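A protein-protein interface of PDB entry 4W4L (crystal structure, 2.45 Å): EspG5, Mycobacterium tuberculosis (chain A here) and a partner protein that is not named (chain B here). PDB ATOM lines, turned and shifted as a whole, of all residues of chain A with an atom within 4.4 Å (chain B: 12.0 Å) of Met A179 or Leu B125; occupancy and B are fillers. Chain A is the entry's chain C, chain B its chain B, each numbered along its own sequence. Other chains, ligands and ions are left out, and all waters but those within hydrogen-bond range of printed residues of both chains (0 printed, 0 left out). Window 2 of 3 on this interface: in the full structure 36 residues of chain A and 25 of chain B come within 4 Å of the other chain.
The backbone NH (N) of Leu A268 is in hydrogen-bond range of the backbone carbonyl oxygen (O) of Val A174. The backbone carbonyl oxygen of Leu B125 is in hydrogen-bond range of the side-chain amide nitrogen of Gln B127, 3.0 Å away. The side-chain amide oxygen (OD1) of Asn B123 sits at hydrogen-bond distance from the backbone NH (N) of Gln B127 (3.4 Å). The backbone carbonyl oxygen of Met A179 lies within hydrogen-bond range of the side-chain hydroxyl of Thr A183, 2.6 Å away. The backbone carbonyl oxygen (O) of Leu A254 sits at hydrogen-bond distance from the backbone NH (N) of Ser A243, 2.9 Å away.
Of the 18 printed residues of chain A, 7 touch a printed residue of chain B. Printed residues of chain A that touch a printed residue of chain B: Met A176, Met A179, Leu A180, Thr A183, Ser A243, Leu A254 and Leu A268. Hydrophobic or aromatic side chains of chain A within 4 Å of the printed part of chain B: Met A176, Met A179, Leu A180, Leu A254 and Leu A268. Of the 16 printed residues of chain B, 2 touch a printed residue of chain A. Printed residues of chain B that touch a printed residue of chain A: Leu B125 and Gln B127. Hydrophobic or aromatic side chains of chain B that line the printed part of chain A: Leu B125. Along chain B the printed residues that touch a printed residue of chain A span positions 125 to 127.
Of the printed residues of chain B, Met A179 touches Leu B125. Of chain A, only Met A179 (3.6 Å), Leu A180 (3.8 Å), Thr A183 (3.6 Å), Ser A243 (3.9 Å), Leu A254 (3.9 Å) and Leu A268 (3.8 Å) come within 4 Å of Leu B125. No residue of chain B comes within 4 Å of Val A174. No residue of chain B comes within 4 Å of Ala A182. Thr A183 touches just one residue of chain B: Leu B125. No residue of chain B comes within 4 Å of Leu A199. Of chain B, only Leu B125 comes within 4 Å of Ser A243. Leu A268 touches one residue of chain B. Of the printed residues of chain A, Gln B127 touches Met A176 and Leu A254. The nearest printed residue of chain A that does not touch Leu B125 is Leu A212 (4.9 Å).
CE of Met A176 touches CG of Gln B127, at 3.5 Å. Met A179 touches Leu B125. CD2 of Leu A180 touches CD1 of Leu B125, at 3.8 Å. OG1 of Thr A183 touches CD1 of Leu B125, 3.6 Å away. Leu B125 touches Ser A243 (O to CB, 3.9 Å). Leu B125 touches Leu A254. O of Leu A254 touches NE2 of Gln B127, 3.5 Å away. Leu B125 touches Leu A268 (CD1 to CD2, 3.8 Å).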
ATOM      1  N   VAL A 174      21.556  -0.873  18.443  1.00  0.00           N
ATOM      2  CA  VAL A 174      21.007  -0.736  19.787  1.00  0.00           C
ATOM      3  C   VAL A 174      19.959  -1.823  20.012  1.00  0.00           C
ATOM      4  O   VAL A 174      19.221  -2.151  19.095  1.00  0.00           O
ATOM      5  CB  VAL A 174      20.390   0.677  19.980  1.00  0.00           C
ATOM      6  CG1 VAL A 174      19.426   0.725  21.157  1.00  0.00           C
ATOM      7  CG2 VAL A 174      21.488   1.718  20.134  1.00  0.00           C
ATOM      8  N   PRO A 175      19.901  -2.401  21.224  1.00  0.00           N
ATOM      9  CA  PRO A 175      18.883  -3.417  21.524  1.00  0.00           C
ATOM     10  C   PRO A 175      17.459  -2.946  21.219  1.00  0.00           C
ATOM     11  O   PRO A 175      17.067  -1.844  21.602  1.00  0.00           O
ATOM     12  CB  PRO A 175      19.068  -3.672  23.028  1.00  0.00           C
ATOM     13  CG  PRO A 175      19.984  -2.576  23.519  1.00  0.00           C
ATOM     14  CD  PRO A 175      20.834  -2.222  22.346  1.00  0.00           C
ATOM     15  N   MET A 176      16.701  -3.798  20.535  1.00  0.00           N
ATOM     16  CA  MET A 176      15.405  -3.440  19.966  1.00  0.00           C
ATOM     17  C   MET A 176      14.350  -2.971  20.970  1.00  0.00           C
ATOM     18  O   MET A 176      13.807  -1.875  20.836  1.00  0.00           O
ATOM     19  CB  MET A 176      14.848  -4.630  19.183  1.00  0.00           C
ATOM     20  CG  MET A 176      13.516  -4.355  18.518  1.00  0.00           C
ATOM     21  SD  MET A 176      13.608  -2.973  17.367  1.00  0.00           S
ATOM     22  CE  MET A 176      11.869  -2.724  17.036  1.00  0.00           C
ATOM     23  N   GLU A 177      14.046  -3.798  21.963  1.00  0.00           N
ATOM     24  CA  GLU A 177      12.959  -3.478  22.885  1.00  0.00           C
ATOM     25  C   GLU A 177      13.312  -2.321  23.818  1.00  0.00           C
ATOM     26  O   GLU A 177      12.445  -1.521  24.179  1.00  0.00           O
ATOM     27  CB  GLU A 177      12.566  -4.712  23.696  1.00  0.00           C
ATOM     28  CG  GLU A 177      13.737  -5.504  24.234  1.00  0.00           C
ATOM     29  CD  GLU A 177      13.298  -6.772  24.939  1.00  0.00           C
ATOM     30  OE1 GLU A 177      14.169  -7.604  25.269  1.00  0.00           O
ATOM     31  OE2 GLU A 177      12.078  -6.935  25.162  1.00  0.00           O
ATOM     32  N   GLU A 178      14.582  -2.234  24.204  1.00  0.00           N
ATOM     33  CA  GLU A 178      15.059  -1.124  25.022  1.00  0.00           C
ATOM     34  C   GLU A 178      14.879   0.175  24.254  1.00  0.00           C
ATOM     35  O   GLU A 178      14.442   1.193  24.805  1.00  0.00           O
ATOM     36  CB  GLU A 178      16.528  -1.316  25.413  1.00  0.00           C
ATOM     37  CG  GLU A 178      16.772  -2.366  26.493  1.00  0.00           C
ATOM     38  CD  GLU A 178      16.480  -3.782  26.026  1.00  0.00           C
ATOM     39  OE1 GLU A 178      16.490  -4.024  24.800  1.00  0.00           O
ATOM     40  OE2 GLU A 178      16.237  -4.656  26.886  1.00  0.00           O
ATOM     41  N   MET A 179      15.212   0.117  22.968  1.00  0.00           N
ATOM     42  CA  MET A 179      15.063   1.258  22.082  1.00  0.00           C
ATOM     43  C   MET A 179      13.596   1.648  21.939  1.00  0.00           C
ATOM     44  O   MET A 179      13.263   2.831  21.926  1.00  0.00           O
ATOM     45  CB  MET A 179      15.666   0.950  20.712  1.00  0.00           C
ATOM     46  CG  MET A 179      15.627   2.120  19.752  1.00  0.00           C
ATOM     47  SD  MET A 179      16.443   3.579  20.418  1.00  0.00           S
ATOM     48  CE  MET A 179      16.040   4.798  19.168  1.00  0.00           C
ATOM     49  N   LEU A 180      12.726   0.645  21.833  1.00  0.00           N
ATOM     50  CA  LEU A 180      11.288   0.882  21.739  1.00  0.00           C
ATOM     51  C   LEU A 180      10.748   1.578  22.978  1.00  0.00           C
ATOM     52  O   LEU A 180       9.970   2.524  22.877  1.00  0.00           O
ATOM     53  CB  LEU A 180      10.536  -0.432  21.527  1.00  0.00           C
ATOM     54  CG  LEU A 180      10.690  -1.084  20.156  1.00  0.00           C
ATOM     55  CD1 LEU A 180       9.935  -2.400  20.112  1.00  0.00           C
ATOM     56  CD2 LEU A 180      10.208  -0.139  19.064  1.00  0.00           C
ATOM     57  N   GLU A 181      11.156   1.101  24.146  1.00  0.00           N
ATOM     58  CA  GLU A 181      10.687   1.677  25.400  1.00  0.00           C
ATOM     59  C   GLU A 181      11.183   3.115  25.568  1.00  0.00           C
ATOM     60  O   GLU A 181      10.409   4.024  25.901  1.00  0.00           O
ATOM     61  CB  GLU A 181      11.138   0.813  26.577  1.00  0.00           C
ATOM     62  CG  GLU A 181      10.524   1.195  27.912  1.00  0.00           C
ATOM     63  CD  GLU A 181      10.459   0.022  28.874  1.00  0.00           C
ATOM     64  OE1 GLU A 181      10.590  -1.134  28.414  1.00  0.00           O
ATOM     65  OE2 GLU A 181      10.277   0.253  30.089  1.00  0.00           O
ATOM     66  N   ALA A 182      12.476   3.313  25.323  1.00  0.00           N
ATOM     67  CA  ALA A 182      13.080   4.637  25.435  1.00  0.00           C
ATOM     68  C   ALA A 182      12.434   5.620  24.468  1.00  0.00           C
ATOM     69  O   ALA A 182      12.172   6.769  24.821  1.00  0.00           O
ATOM     70  CB  ALA A 182      14.574   4.560  25.185  1.00  0.00           C
ATOM     71  N   THR A 183      12.178   5.159  23.249  1.00  0.00           N
ATOM     72  CA  THR A 183      11.561   5.994  22.231  1.00  0.00           C
ATOM     73  C   THR A 183      10.118   6.304  22.596  1.00  0.00           C
ATOM     74  O   THR A 183       9.623   7.398  22.328  1.00  0.00           O
ATOM     75  CB  THR A 183      11.602   5.326  20.849  1.00  0.00           C
ATOM     76  OG1 THR A 183      12.958   5.011  20.514  1.00  0.00           O
ATOM     77  CG2 THR A 183      11.032   6.254  19.790  1.00  0.00           C
ATOM     78  N   LEU A 199      18.352   7.755  25.637  1.00  0.00           N
ATOM     79  CA  LEU A 199      18.972   7.263  24.413  1.00  0.00           C
ATOM     80  C   LEU A 199      20.481   7.489  24.438  1.00  0.00           C
ATOM     81  O   LEU A 199      21.242   6.712  23.862  1.00  0.00           O
ATOM     82  CB  LEU A 199      18.349   7.933  23.184  1.00  0.00           C
ATOM     83  CG  LEU A 199      17.000   7.372  22.718  1.00  0.00           C
ATOM     84  CD1 LEU A 199      15.855   7.784  23.636  1.00  0.00           C
ATOM     85  CD2 LEU A 199      16.711   7.777  21.280  1.00  0.00           C
ATOM     86  N   MET A 202      22.128   4.696  26.293  1.00  0.00           N
ATOM     87  CA  MET A 202      22.254   3.473  25.503  1.00  0.00           C
ATOM     88  C   MET A 202      23.493   3.474  24.611  1.00  0.00           C
ATOM     89  O   MET A 202      23.794   2.472  23.963  1.00  0.00           O
ATOM     90  CB  MET A 202      21.009   3.259  24.641  1.00  0.00           C
ATOM     91  CG  MET A 202      19.800   2.751  25.405  1.00  0.00           C
ATOM     92  SD  MET A 202      18.466   2.244  24.302  1.00  0.00           S
ATOM     93  CE  MET A 202      18.044   3.815  23.561  1.00  0.00           C
ATOM     94  N   ILE A 204      24.087   5.959  22.221  1.00  0.00           N
ATOM     95  CA  ILE A 204      23.817   6.655  20.972  1.00  0.00           C
ATOM     96  C   ILE A 204      24.430   8.056  21.029  1.00  0.00           C
ATOM     97  O   ILE A 204      24.338   8.733  22.053  1.00  0.00           O
ATOM     98  CB  ILE A 204      22.307   6.737  20.702  1.00  0.00           C
ATOM     99  CG1 ILE A 204      21.660   5.364  20.910  1.00  0.00           C
ATOM    100  CG2 ILE A 204      22.040   7.239  19.302  1.00  0.00           C
ATOM    101  CD1 ILE A 204      20.153   5.372  20.793  1.00  0.00           C
ATOM    102  N   LEU A 212      17.829  12.161  14.938  1.00  0.00           N
ATOM    103  CA  LEU A 212      16.693  11.261  15.102  1.00  0.00           C
ATOM    104  C   LEU A 212      15.534  11.984  15.770  1.00  0.00           C
ATOM    105  O   LEU A 212      14.377  11.777  15.424  1.00  0.00           O
ATOM    106  CB  LEU A 212      17.097  10.033  15.922  1.00  0.00           C
ATOM    107  CG  LEU A 212      16.030   8.976  16.199  1.00  0.00           C
ATOM    108  CD1 LEU A 212      15.417   8.473  14.899  1.00  0.00           C
ATOM    109  CD2 LEU A 212      16.630   7.825  16.992  1.00  0.00           C
ATOM    110  N   SER A 243      13.105   2.010   7.571  1.00  0.00           N
ATOM    111  CA  SER A 243      12.416   3.288   7.652  1.00  0.00           C
ATOM    112  C   SER A 243      13.358   4.448   7.369  1.00  0.00           C
ATOM    113  O   SER A 243      14.319   4.671   8.096  1.00  0.00           O
ATOM    114  CB  SER A 243      11.772   3.465   9.024  1.00  0.00           C
ATOM    115  OG  SER A 243      11.017   4.663   9.069  1.00  0.00           O
ATOM    116  N   LEU A 254      16.479   3.435   9.538  1.00  0.00           N
ATOM    117  CA  LEU A 254      16.281   2.579  10.704  1.00  0.00           C
ATOM    118  C   LEU A 254      15.852   1.182  10.276  1.00  0.00           C
ATOM    119  O   LEU A 254      14.796   1.022   9.676  1.00  0.00           O
ATOM    120  CB  LEU A 254      15.224   3.171  11.638  1.00  0.00           C
ATOM    121  CG  LEU A 254      15.406   4.606  12.125  1.00  0.00           C
ATOM    122  CD1 LEU A 254      14.152   5.070  12.843  1.00  0.00           C
ATOM    123  CD2 LEU A 254      16.613   4.705  13.034  1.00  0.00           C
ATOM    124  N   LEU A 268      18.388  -3.139  16.557  1.00  0.00           N
ATOM    125  CA  LEU A 268      17.965  -2.056  15.680  1.00  0.00           C
ATOM    126  C   LEU A 268      19.164  -1.245  15.215  1.00  0.00           C
ATOM    127  O   LEU A 268      19.955  -0.757  16.024  1.00  0.00           O
ATOM    128  CB  LEU A 268      16.958  -1.137  16.376  1.00  0.00           C
ATOM    129  CG  LEU A 268      16.483   0.023  15.496  1.00  0.00           C
ATOM    130  CD1 LEU A 268      15.738  -0.500  14.272  1.00  0.00           C
ATOM    131  CD2 LEU A 268      15.621   1.005  16.275  1.00  0.00           C
ATOM    132  N   ILE A 270      20.567   2.040  13.569  1.00  0.00           N
ATOM    133  CA  ILE A 270      20.352   3.454  13.318  1.00  0.00           C
ATOM    134  C   ILE A 270      21.511   3.967  12.472  1.00  0.00           C
ATOM    135  O   ILE A 270      22.653   4.016  12.933  1.00  0.00           O
ATOM    136  CB  ILE A 270      20.255   4.250  14.631  1.00  0.00           C
ATOM    137  CG1 ILE A 270      19.258   3.584  15.579  1.00  0.00           C
ATOM    138  CG2 ILE A 270      19.873   5.695  14.360  1.00  0.00           C
ATOM    139  CD1 ILE A 270      19.268   4.163  16.975  1.00  0.00           C
ATOM    140  N   GLN B 117      -4.523   0.356  15.811  1.00  0.00           N
ATOM    141  CA  GLN B 117      -4.258   1.689  16.348  1.00  0.00           C
ATOM    142  C   GLN B 117      -3.153   1.665  17.407  1.00  0.00           C
ATOM    143  O   GLN B 117      -2.290   2.552  17.430  1.00  0.00           O
ATOM    144  CB  GLN B 117      -5.536   2.301  16.933  1.00  0.00           C
ATOM    145  CG  GLN B 117      -5.441   3.804  17.175  1.00  0.00           C
ATOM    146  CD  GLN B 117      -5.027   4.576  15.929  1.00  0.00           C
ATOM    147  OE1 GLN B 117      -5.689   4.512  14.891  1.00  0.00           O
ATOM    148  NE2 GLN B 117      -3.919   5.310  16.029  1.00  0.00           N
ATOM    149  N   ILE B 118      -3.179   0.651  18.272  1.00  0.00           N
ATOM    150  CA  ILE B 118      -2.103   0.480  19.249  1.00  0.00           C
ATOM    151  C   ILE B 118      -0.747   0.353  18.556  1.00  0.00           C
ATOM    152  O   ILE B 118       0.234   0.970  18.988  1.00  0.00           O
ATOM    153  CB  ILE B 118      -2.328  -0.750  20.153  1.00  0.00           C
ATOM    154  CG1 ILE B 118      -3.394  -0.450  21.205  1.00  0.00           C
ATOM    155  CG2 ILE B 118      -1.038  -1.145  20.861  1.00  0.00           C
ATOM    156  CD1 ILE B 118      -3.780  -1.666  22.035  1.00  0.00           C
ATOM    157  N   LEU B 119      -0.686  -0.429  17.479  1.00  0.00           N
ATOM    158  CA  LEU B 119       0.565  -0.544  16.724  1.00  0.00           C
ATOM    159  C   LEU B 119       0.980   0.802  16.129  1.00  0.00           C
ATOM    160  O   LEU B 119       2.160   1.167  16.165  1.00  0.00           O
ATOM    161  CB  LEU B 119       0.445  -1.593  15.618  1.00  0.00           C
ATOM    162  CG  LEU B 119       0.266  -3.035  16.093  1.00  0.00           C
ATOM    163  CD1 LEU B 119       0.411  -4.014  14.938  1.00  0.00           C
ATOM    164  CD2 LEU B 119       1.253  -3.362  17.201  1.00  0.00           C
ATOM    165  N   ILE B 120       0.011   1.542  15.589  1.00  0.00           N
ATOM    166  CA  ILE B 120       0.284   2.864  15.029  1.00  0.00           C
ATOM    167  C   ILE B 120       0.928   3.785  16.065  1.00  0.00           C
ATOM    168  O   ILE B 120       1.965   4.394  15.801  1.00  0.00           O
ATOM    169  CB  ILE B 120      -0.994   3.536  14.499  1.00  0.00           C
ATOM    170  CG1 ILE B 120      -1.564   2.748  13.318  1.00  0.00           C
ATOM    171  CG2 ILE B 120      -0.704   4.971  14.070  1.00  0.00           C
ATOM    172  CD1 ILE B 120      -0.787   2.925  12.039  1.00  0.00           C
ATOM    173  N   ASP B 121       0.317   3.870  17.245  1.00  0.00           N
ATOM    174  CA  ASP B 121       0.828   4.729  18.313  1.00  0.00           C
ATOM    175  C   ASP B 121       2.282   4.418  18.676  1.00  0.00           C
ATOM    176  O   ASP B 121       3.046   5.303  19.061  1.00  0.00           O
ATOM    177  CB  ASP B 121      -0.045   4.599  19.562  1.00  0.00           C
ATOM    178  CG  ASP B 121      -1.488   4.985  19.310  1.00  0.00           C
ATOM    179  OD1 ASP B 121      -1.744   5.774  18.377  1.00  0.00           O
ATOM    180  OD2 ASP B 121      -2.369   4.501  20.053  1.00  0.00           O
ATOM    181  N   ASN B 122       2.643   3.145  18.567  1.00  0.00           N
ATOM    182  CA  ASN B 122       3.977   2.660  18.903  1.00  0.00           C
ATOM    183  C   ASN B 122       4.936   2.562  17.718  1.00  0.00           C
ATOM    184  O   ASN B 122       6.021   2.001  17.841  1.00  0.00           O
ATOM    185  CB  ASN B 122       3.874   1.307  19.600  1.00  0.00           C
ATOM    186  CG  ASN B 122       3.503   1.443  21.060  1.00  0.00           C
ATOM    187  OD1 ASN B 122       4.369   1.636  21.916  1.00  0.00           O
ATOM    188  ND2 ASN B 122       2.209   1.356  21.353  1.00  0.00           N
ATOM    189  N   ASN B 123       4.513   3.058  16.560  1.00  0.00           N
ATOM    190  CA  ASN B 123       5.248   2.846  15.315  1.00  0.00           C
ATOM    191  C   ASN B 123       6.310   3.897  14.969  1.00  0.00           C
ATOM    192  O   ASN B 123       6.821   3.905  13.847  1.00  0.00           O
ATOM    193  CB  ASN B 123       4.283   2.713  14.140  1.00  0.00           C
ATOM    194  CG  ASN B 123       4.881   1.909  13.005  1.00  0.00           C
ATOM    195  OD1 ASN B 123       5.797   1.118  13.217  1.00  0.00           O
ATOM    196  ND2 ASN B 123       4.382   2.118  11.796  1.00  0.00           N
ATOM    197  N   ALA B 124       6.607   4.804  15.897  1.00  0.00           N
ATOM    198  CA  ALA B 124       7.560   5.887  15.639  1.00  0.00           C
ATOM    199  C   ALA B 124       8.836   5.391  14.953  1.00  0.00           C
ATOM    200  O   ALA B 124       9.378   6.075  14.088  1.00  0.00           O
ATOM    201  CB  ALA B 124       7.915   6.600  16.935  1.00  0.00           C
ATOM    202  N   LEU B 125       9.311   4.207  15.330  1.00  0.00           N
ATOM    203  CA  LEU B 125      10.513   3.647  14.715  1.00  0.00           C
ATOM    204  C   LEU B 125      10.203   2.847  13.449  1.00  0.00           C
ATOM    205  O   LEU B 125      11.116   2.416  12.743  1.00  0.00           O
ATOM    206  CB  LEU B 125      11.264   2.770  15.716  1.00  0.00           C
ATOM    207  CG  LEU B 125      11.825   3.526  16.920  1.00  0.00           C
ATOM    208  CD1 LEU B 125      12.560   2.580  17.853  1.00  0.00           C
ATOM    209  CD2 LEU B 125      12.738   4.650  16.460  1.00  0.00           C
ATOM    210  N   GLY B 126       8.920   2.641  13.171  1.00  0.00           N
ATOM    211  CA  GLY B 126       8.493   2.038  11.919  1.00  0.00           C
ATOM    212  C   GLY B 126       8.506   0.522  11.835  1.00  0.00           C
ATOM    213  O   GLY B 126       8.141  -0.046  10.804  1.00  0.00           O
ATOM    214  N   GLN B 127       8.901  -0.143  12.915  1.00  0.00           N
ATOM    215  CA  GLN B 127       9.109  -1.588  12.872  1.00  0.00           C
ATOM    216  C   GLN B 127       7.831  -2.422  12.995  1.00  0.00           C
ATOM    217  O   GLN B 127       7.866  -3.643  12.832  1.00  0.00           O
ATOM    218  CB  GLN B 127      10.096  -1.994  13.965  1.00  0.00           C
ATOM    219  CG  GLN B 127      11.430  -1.297  13.837  1.00  0.00           C
ATOM    220  CD  GLN B 127      11.989  -1.380  12.428  1.00  0.00           C
ATOM    221  OE1 GLN B 127      12.136  -2.468  11.869  1.00  0.00           O
ATOM    222  NE2 GLN B 127      12.288  -0.225  11.841  1.00  0.00           N
ATOM    223  N   PHE B 128       6.710  -1.775  13.292  1.00  0.00           N
ATOM    224  CA  PHE B 128       5.433  -2.481  13.387  1.00  0.00           C
ATOM    225  C   PHE B 128       4.628  -2.420  12.092  1.00  0.00           C
ATOM    226  O   PHE B 128       3.496  -2.899  12.035  1.00  0.00           O
ATOM    227  CB  PHE B 128       4.604  -1.924  14.543  1.00  0.00           C
ATOM    228  CG  PHE B 128       5.182  -2.222  15.892  1.00  0.00           C
ATOM    229  CD1 PHE B 128       5.251  -3.527  16.354  1.00  0.00           C
ATOM    230  CD2 PHE B 128       5.656  -1.204  16.701  1.00  0.00           C
ATOM    231  CE1 PHE B 128       5.784  -3.810  17.597  1.00  0.00           C
ATOM    232  CE2 PHE B 128       6.191  -1.481  17.948  1.00  0.00           C
ATOM    233  CZ  PHE B 128       6.256  -2.784  18.395  1.00  0.00           C
ATOM    234  N   THR B 129       5.216  -1.822  11.063  1.00  0.00           N
ATOM    235  CA  THR B 129       4.507  -1.487   9.827  1.00  0.00           C
ATOM    236  C   THR B 129       3.927  -2.708   9.108  1.00  0.00           C
ATOM    237  O   THR B 129       2.754  -2.711   8.691  1.00  0.00           O
ATOM    238  CB  THR B 129       5.447  -0.722   8.867  1.00  0.00           C
ATOM    239  OG1 THR B 129       6.104   0.331   9.585  1.00  0.00           O
ATOM    240  CG2 THR B 129       4.673  -0.127   7.701  1.00  0.00           C
ATOM    241  N   ALA B 130       4.742  -3.748   8.971  1.00  0.00           N
ATOM    242  CA  ALA B 130       4.295  -4.977   8.328  1.00  0.00           C
ATOM    243  C   ALA B 130       3.141  -5.617   9.103  1.00  0.00           C
ATOM    244  O   ALA B 130       2.208  -6.154   8.508  1.00  0.00           O
ATOM    245  CB  ALA B 130       5.454  -5.952   8.187  1.00  0.00           C
ATOM    246  N   GLN B 131       3.199  -5.547  10.430  1.00  0.00           N
ATOM    247  CA  GLN B 131       2.137  -6.106  11.260  1.00  0.00           C
ATOM    248  C   GLN B 131       0.835  -5.334  11.055  1.00  0.00           C
ATOM    249  O   GLN B 131      -0.249  -5.919  11.011  1.00  0.00           O
ATOM    250  CB  GLN B 131       2.542  -6.092  12.735  1.00  0.00           C
ATOM    251  CG  GLN B 131       3.719  -7.002  13.049  1.00  0.00           C
ATOM    252  CD  GLN B 131       4.094  -7.002  14.521  1.00  0.00           C
ATOM    253  OE1 GLN B 131       3.328  -6.546  15.370  1.00  0.00           O
ATOM    254  NE2 GLN B 131       5.279  -7.514  14.827  1.00  0.00           N
ATOM    255  N   ILE B 132       0.956  -4.020  10.924  1.00  0.00           N
ATOM    256  CA  ILE B 132      -0.178  -3.156  10.623  1.00  0.00           C
ATOM    257  C   ILE B 132      -0.806  -3.567   9.295  1.00  0.00           C
ATOM    258  O   ILE B 132      -2.037  -3.702   9.183  1.00  0.00           O
ATOM    259  CB  ILE B 132       0.251  -1.677  10.580  1.00  0.00           C
ATOM    260  CG1 ILE B 132       0.736  -1.234  11.962  1.00  0.00           C
ATOM    261  CG2 ILE B 132      -0.890  -0.796  10.110  1.00  0.00           C
ATOM    262  CD1 ILE B 132       1.480   0.085  11.966  1.00  0.00           C
